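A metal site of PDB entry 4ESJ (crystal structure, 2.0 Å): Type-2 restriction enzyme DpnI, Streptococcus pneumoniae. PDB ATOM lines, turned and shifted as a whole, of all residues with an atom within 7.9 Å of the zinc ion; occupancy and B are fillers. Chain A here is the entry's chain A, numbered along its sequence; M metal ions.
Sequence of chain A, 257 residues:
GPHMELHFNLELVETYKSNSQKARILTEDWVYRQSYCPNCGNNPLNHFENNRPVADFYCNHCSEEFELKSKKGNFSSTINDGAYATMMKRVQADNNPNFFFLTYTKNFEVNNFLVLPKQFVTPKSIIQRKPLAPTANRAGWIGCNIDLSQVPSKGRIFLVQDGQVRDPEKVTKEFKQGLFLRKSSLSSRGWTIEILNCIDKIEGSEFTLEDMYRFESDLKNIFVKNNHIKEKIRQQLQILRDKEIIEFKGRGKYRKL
The side-chain sulfur (SG) of Cys 59 lies close to the side-chain amide nitrogen (ND2) of Asn 42 (3.2 Å). The backbone carbonyl oxygen (O) of Glu 64 is in hydrogen-bond range of the backbone NH (N) of Cys 59 (2.9 Å). SG of Cys 37 sits close to N of Asn 39, at 3.5 Å. The backbone carbonyl oxygen (O) of Asn 42 lies within hydrogen-bond range of the backbone NH (N) of Cys 37 (2.8 Å). SG of Cys 59 sits close to N of His 61 (3.5 Å). The side-chain sulfur of Cys 62 sits close to the side-chain amide nitrogen of Asn 39. The side-chain sulfur of Cys 40 lies close to the backbone NH of Asn 42 (3.6 Å). The side-chain sulfur of Cys 62 lies close to the backbone NH of Glu 64, at 3.7 Å.
Four residues have an atom within 4 Å of the zinc ion: Cys 37, Cys 40, Cys 59 and Cys 62. The nearest printed residue that does not touch the zinc ion is Asn 42 (4.3 Å).
The zinc ion is bound by SG of Cys 62 (2.3 Å), SG of Cys 59 (2.3 Å), SG of Cys 40 (2.3 Å) and SG of Cys 37 (2.3 Å).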
ATOM      1  N   TYR A  36      27.817  29.421  -7.364  1.00  0.00           N
ATOM      2  CA  TYR A  36      26.829  28.543  -6.797  1.00  0.00           C
ATOM      3  C   TYR A  36      25.521  28.813  -7.527  1.00  0.00           C
ATOM      4  O   TYR A  36      25.379  29.860  -8.149  1.00  0.00           O
ATOM      5  CB  TYR A  36      26.676  28.797  -5.289  1.00  0.00           C
ATOM      6  CG  TYR A  36      26.378  30.238  -4.885  1.00  0.00           C
ATOM      7  CD1 TYR A  36      27.412  31.123  -4.582  1.00  0.00           C
ATOM      8  CD2 TYR A  36      25.060  30.712  -4.758  1.00  0.00           C
ATOM      9  CE1 TYR A  36      27.153  32.417  -4.187  1.00  0.00           C
ATOM     10  CE2 TYR A  36      24.788  32.022  -4.374  1.00  0.00           C
ATOM     11  CZ  TYR A  36      25.833  32.871  -4.096  1.00  0.00           C
ATOM     12  OH  TYR A  36      25.602  34.164  -3.701  1.00  0.00           O
ATOM     13  N   CYS A  37      24.567  27.887  -7.420  1.00  0.00           N
ATOM     14  CA  CYS A  37      23.256  28.101  -8.004  1.00  0.00           C
ATOM     15  C   CYS A  37      22.495  29.165  -7.220  1.00  0.00           C
ATOM     16  O   CYS A  37      22.235  28.999  -6.022  1.00  0.00           O
ATOM     17  CB  CYS A  37      22.459  26.825  -7.990  1.00  0.00           C
ATOM     18  SG  CYS A  37      20.827  27.036  -8.690  1.00  0.00           S
ATOM     19  N   PRO A  38      22.173  30.282  -7.881  1.00  0.00           N
ATOM     20  CA  PRO A  38      21.469  31.362  -7.195  1.00  0.00           C
ATOM     21  C   PRO A  38      20.004  31.070  -6.902  1.00  0.00           C
ATOM     22  O   PRO A  38      19.397  31.843  -6.199  1.00  0.00           O
ATOM     23  CB  PRO A  38      21.646  32.558  -8.137  1.00  0.00           C
ATOM     24  CG  PRO A  38      21.744  31.927  -9.497  1.00  0.00           C
ATOM     25  CD  PRO A  38      22.502  30.643  -9.283  1.00  0.00           C
ATOM     26  N   ASN A  39      19.454  29.969  -7.408  1.00  0.00           N
ATOM     27  CA  ASN A  39      18.137  29.456  -6.983  1.00  0.00           C
ATOM     28  C   ASN A  39      18.211  28.700  -5.633  1.00  0.00           C
ATOM     29  O   ASN A  39      17.617  29.121  -4.648  1.00  0.00           O
ATOM     30  CB  ASN A  39      17.564  28.525  -8.059  1.00  0.00           C
ATOM     31  CG  ASN A  39      16.107  28.151  -7.806  1.00  0.00           C
ATOM     32  OD1 ASN A  39      15.316  28.959  -7.302  1.00  0.00           O
ATOM     33  ND2 ASN A  39      15.742  26.935  -8.191  1.00  0.00           N
ATOM     34  N   CYS A  40      18.974  27.607  -5.589  1.00  0.00           N
ATOM     35  CA  CYS A  40      18.970  26.701  -4.443  1.00  0.00           C
ATOM     36  C   CYS A  40      20.276  26.686  -3.656  1.00  0.00           C
ATOM     37  O   CYS A  40      20.340  26.038  -2.613  1.00  0.00           O
ATOM     38  CB  CYS A  40      18.659  25.287  -4.919  1.00  0.00           C
ATOM     39  SG  CYS A  40      20.050  24.504  -5.787  1.00  0.00           S
ATOM     40  N   GLY A  41      21.316  27.386  -4.136  1.00  0.00           N
ATOM     41  CA  GLY A  41      22.576  27.516  -3.393  1.00  0.00           C
ATOM     42  C   GLY A  41      23.610  26.399  -3.613  1.00  0.00           C
ATOM     43  O   GLY A  41      24.728  26.472  -3.089  1.00  0.00           O
ATOM     44  N   ASN A  42      23.212  25.389  -4.379  1.00  0.00           N
ATOM     45  CA  ASN A  42      24.065  24.241  -4.721  1.00  0.00           C
ATOM     46  C   ASN A  42      25.408  24.666  -5.374  1.00  0.00           C
ATOM     47  O   ASN A  42      25.431  25.506  -6.281  1.00  0.00           O
ATOM     48  CB  ASN A  42      23.247  23.322  -5.670  1.00  0.00           C
ATOM     49  CG  ASN A  42      24.020  22.085  -6.146  1.00  0.00           C
ATOM     50  OD1 ASN A  42      24.719  21.442  -5.376  1.00  0.00           O
ATOM     51  ND2 ASN A  42      23.858  21.741  -7.419  1.00  0.00           N
ATOM     52  N   ASN A  43      26.528  24.106  -4.878  1.00  0.00           N
ATOM     53  CA  ASN A  43      27.890  24.304  -5.446  1.00  0.00           C
ATOM     54  C   ASN A  43      28.634  22.966  -5.390  1.00  0.00           C
ATOM     55  O   ASN A  43      28.538  22.263  -4.367  1.00  0.00           O
ATOM     56  CB  ASN A  43      28.698  25.408  -4.714  1.00  0.00           C
ATOM     57  CG  ASN A  43      30.238  25.376  -5.033  1.00  0.00           C
ATOM     58  OD1 ASN A  43      31.008  24.582  -4.473  1.00  0.00           O
ATOM     59  ND2 ASN A  43      30.700  26.296  -5.903  1.00  0.00           N
ATOM     60  N   LEU A  45      28.223  23.884  -9.716  1.00  0.00           N
ATOM     61  CA  LEU A  45      27.377  23.685 -10.877  1.00  0.00           C
ATOM     62  C   LEU A  45      27.968  22.637 -11.807  1.00  0.00           C
ATOM     63  O   LEU A  45      29.140  22.268 -11.695  1.00  0.00           O
ATOM     64  CB  LEU A  45      27.219  25.010 -11.642  1.00  0.00           C
ATOM     65  CG  LEU A  45      26.467  26.103 -10.885  1.00  0.00           C
ATOM     66  CD1 LEU A  45      26.428  27.426 -11.672  1.00  0.00           C
ATOM     67  CD2 LEU A  45      25.108  25.618 -10.570  1.00  0.00           C
ATOM     68  N   TYR A  58      24.525  24.004 -15.662  1.00  0.00           N
ATOM     69  CA  TYR A  58      23.221  23.714 -15.011  1.00  0.00           C
ATOM     70  C   TYR A  58      23.446  23.253 -13.567  1.00  0.00           C
ATOM     71  O   TYR A  58      24.568  22.833 -13.182  1.00  0.00           O
ATOM     72  CB  TYR A  58      22.390  22.690 -15.792  1.00  0.00           C
ATOM     73  CG  TYR A  58      22.909  21.286 -15.738  1.00  0.00           C
ATOM     74  CD1 TYR A  58      23.917  20.868 -16.599  1.00  0.00           C
ATOM     75  CD2 TYR A  58      22.397  20.355 -14.819  1.00  0.00           C
ATOM     76  CE1 TYR A  58      24.402  19.584 -16.551  1.00  0.00           C
ATOM     77  CE2 TYR A  58      22.897  19.066 -14.758  1.00  0.00           C
ATOM     78  CZ  TYR A  58      23.908  18.694 -15.635  1.00  0.00           C
ATOM     79  OH  TYR A  58      24.422  17.422 -15.628  1.00  0.00           O
ATOM     80  N   CYS A  59      22.391  23.334 -12.790  1.00  0.00           N
ATOM     81  CA  CYS A  59      22.380  22.862 -11.419  1.00  0.00           C
ATOM     82  C   CYS A  59      21.807  21.454 -11.377  1.00  0.00           C
ATOM     83  O   CYS A  59      20.700  21.229 -11.822  1.00  0.00           O
ATOM     84  CB  CYS A  59      21.546  23.791 -10.551  1.00  0.00           C
ATOM     85  SG  CYS A  59      21.508  23.356  -8.791  1.00  0.00           S
ATOM     86  N   ASN A  60      22.580  20.512 -10.848  1.00  0.00           N
ATOM     87  CA  ASN A  60      22.143  19.104 -10.738  1.00  0.00           C
ATOM     88  C   ASN A  60      21.145  18.846  -9.600  1.00  0.00           C
ATOM     89  O   ASN A  60      20.672  17.707  -9.436  1.00  0.00           O
ATOM     90  CB  ASN A  60      23.338  18.115 -10.702  1.00  0.00           C
ATOM     91  CG  ASN A  60      24.189  18.177  -9.406  1.00  0.00           C
ATOM     92  OD1 ASN A  60      23.832  18.823  -8.429  1.00  0.00           O
ATOM     93  ND2 ASN A  60      25.337  17.502  -9.420  1.00  0.00           N
ATOM     94  N   HIS A  61      20.857  19.882  -8.811  1.00  0.00           N
ATOM     95  CA  HIS A  61      19.843  19.807  -7.749  1.00  0.00           C
ATOM     96  C   HIS A  61      18.492  20.309  -8.236  1.00  0.00           C
ATOM     97  O   HIS A  61      17.484  19.610  -8.133  1.00  0.00           O
ATOM     98  CB  HIS A  61      20.301  20.590  -6.506  1.00  0.00           C
ATOM     99  CG  HIS A  61      19.332  20.524  -5.351  1.00  0.00           C
ATOM    100  ND1 HIS A  61      18.990  19.355  -4.721  1.00  0.00           N
ATOM    101  CD2 HIS A  61      18.634  21.507  -4.725  1.00  0.00           C
ATOM    102  CE1 HIS A  61      18.120  19.604  -3.756  1.00  0.00           C
ATOM    103  NE2 HIS A  61      17.884  20.901  -3.745  1.00  0.00           N
ATOM    104  N   CYS A  62      18.469  21.512  -8.816  1.00  0.00           N
ATOM    105  CA  CYS A  62      17.193  22.152  -9.192  1.00  0.00           C
ATOM    106  C   CYS A  62      16.973  22.317 -10.699  1.00  0.00           C
ATOM    107  O   CYS A  62      15.940  22.790 -11.110  1.00  0.00           O
ATOM    108  CB  CYS A  62      17.026  23.498  -8.483  1.00  0.00           C
ATOM    109  SG  CYS A  62      18.074  24.824  -9.220  1.00  0.00           S
ATOM    110  N   SER A  63      17.962  21.927 -11.514  1.00  0.00           N
ATOM    111  CA  SER A  63      17.861  21.966 -12.985  1.00  0.00           C
ATOM    112  C   SER A  63      17.885  23.340 -13.651  1.00  0.00           C
ATOM    113  O   SER A  63      17.804  23.415 -14.874  1.00  0.00           O
ATOM    114  CB  SER A  63      16.620  21.199 -13.476  1.00  0.00           C
ATOM    115  OG  SER A  63      16.681  19.852 -13.053  1.00  0.00           O
ATOM    116  N   GLU A  64      18.011  24.420 -12.904  1.00  0.00           N
ATOM    117  CA  GLU A  64      18.256  25.722 -13.531  1.00  0.00           C
ATOM    118  C   GLU A  64      19.463  25.712 -14.470  1.00  0.00           C
ATOM    119  O   GLU A  64      20.496  25.064 -14.173  1.00  0.00           O
ATOM    120  CB  GLU A  64      18.417  26.834 -12.492  1.00  0.00           C
ATOM    121  CG  GLU A  64      17.105  27.190 -11.757  1.00  0.00           C
ATOM    122  CD  GLU A  64      16.001  27.750 -12.661  1.00  0.00           C
ATOM    123  OE1 GLU A  64      16.246  28.615 -13.536  1.00  0.00           O
ATOM    124  OE2 GLU A  64      14.837  27.323 -12.481  1.00  0.00           O
ATOM    125  N   GLU A  65      19.332  26.419 -15.584  1.00  0.00           N
ATOM    126  CA  GLU A  65      20.402  26.570 -16.570  1.00  0.00           C
ATOM    127  C   GLU A  65      20.920  28.001 -16.605  1.00  0.00           C
ATOM    128  O   GLU A  65      20.170  28.944 -16.406  1.00  0.00           O
ATOM    129  CB  GLU A  65      19.936  26.173 -17.966  1.00  0.00           C
ATOM    130  CG  GLU A  65      19.251  24.804 -17.987  1.00  0.00           C
ATOM    131  CD  GLU A  65      18.853  24.360 -19.383  1.00  0.00           C
ATOM    132  OE1 GLU A  65      19.123  25.099 -20.364  1.00  0.00           O
ATOM    133  OE2 GLU A  65      18.272  23.250 -19.485  1.00  0.00           O
ATOM    134  N   PHE A  66      22.232  28.137 -16.830  1.00  0.00           N
ATOM    135  CA  PHE A  66      22.923  29.413 -16.882  1.00  0.00           C
ATOM    136  C   PHE A  66      23.890  29.459 -18.043  1.00  0.00           C
ATOM    137  O   PHE A  66      24.690  28.534 -18.243  1.00  0.00           O
ATOM    138  CB  PHE A  66      23.669  29.687 -15.602  1.00  0.00           C
ATOM    139  CG  PHE A  66      22.846  29.486 -14.385  1.00  0.00           C
ATOM    140  CD1 PHE A  66      22.731  28.229 -13.802  1.00  0.00           C
ATOM    141  CD2 PHE A  66      22.104  30.565 -13.855  1.00  0.00           C
ATOM    142  CE1 PHE A  66      21.922  28.027 -12.688  1.00  0.00           C
ATOM    143  CE2 PHE A  66      21.303  30.380 -12.728  1.00  0.00           C
ATOM    144  CZ  PHE A  66      21.193  29.096 -12.161  1.00  0.00           C
ATOM    145  N   PHE A 175      16.344  35.726  -5.979  1.00  0.00           N
ATOM    146  CA  PHE A 175      16.058  34.861  -7.135  1.00  0.00           C
ATOM    147  C   PHE A 175      14.664  34.217  -7.011  1.00  0.00           C
ATOM    148  O   PHE A 175      13.842  34.276  -7.928  1.00  0.00           O
ATOM    149  CB  PHE A 175      17.146  33.788  -7.274  1.00  0.00           C
ATOM    150  CG  PHE A 175      17.148  33.096  -8.617  1.00  0.00           C
ATOM    151  CD1 PHE A 175      17.944  33.569  -9.654  1.00  0.00           C
ATOM    152  CD2 PHE A 175      16.353  31.988  -8.840  1.00  0.00           C
ATOM    153  CE1 PHE A 175      17.944  32.939 -10.896  1.00  0.00           C
ATOM    154  CE2 PHE A 175      16.332  31.353 -10.091  1.00  0.00           C
ATOM    155  CZ  PHE A 175      17.128  31.831 -11.111  1.00  0.00           C
ATOM    156  N   LYS A 176      14.379  33.614  -5.855  1.00  0.00           N
ATOM    157  CA  LYS A 176      13.078  32.968  -5.648  1.00  0.00           C
ATOM    158  C   LYS A 176      11.918  33.966  -5.689  1.00  0.00           C
ATOM    159  O   LYS A 176      10.866  33.655  -6.242  1.00  0.00           O
ATOM    160  CB  LYS A 176      13.078  32.188  -4.337  1.00  0.00           C
ATOM    161  CG  LYS A 176      14.108  31.069  -4.313  1.00  0.00           C
ATOM    162  CD  LYS A 176      13.693  29.848  -3.566  1.00  0.00           C
ATOM    163  CE  LYS A 176      14.335  28.580  -4.142  1.00  0.00           C
ATOM    164  NZ  LYS A 176      13.535  28.046  -5.318  1.00  0.00           N
HETATM  165 ZN    ZN M   1      20.026  24.944  -8.050  1.00  0.00          ZN
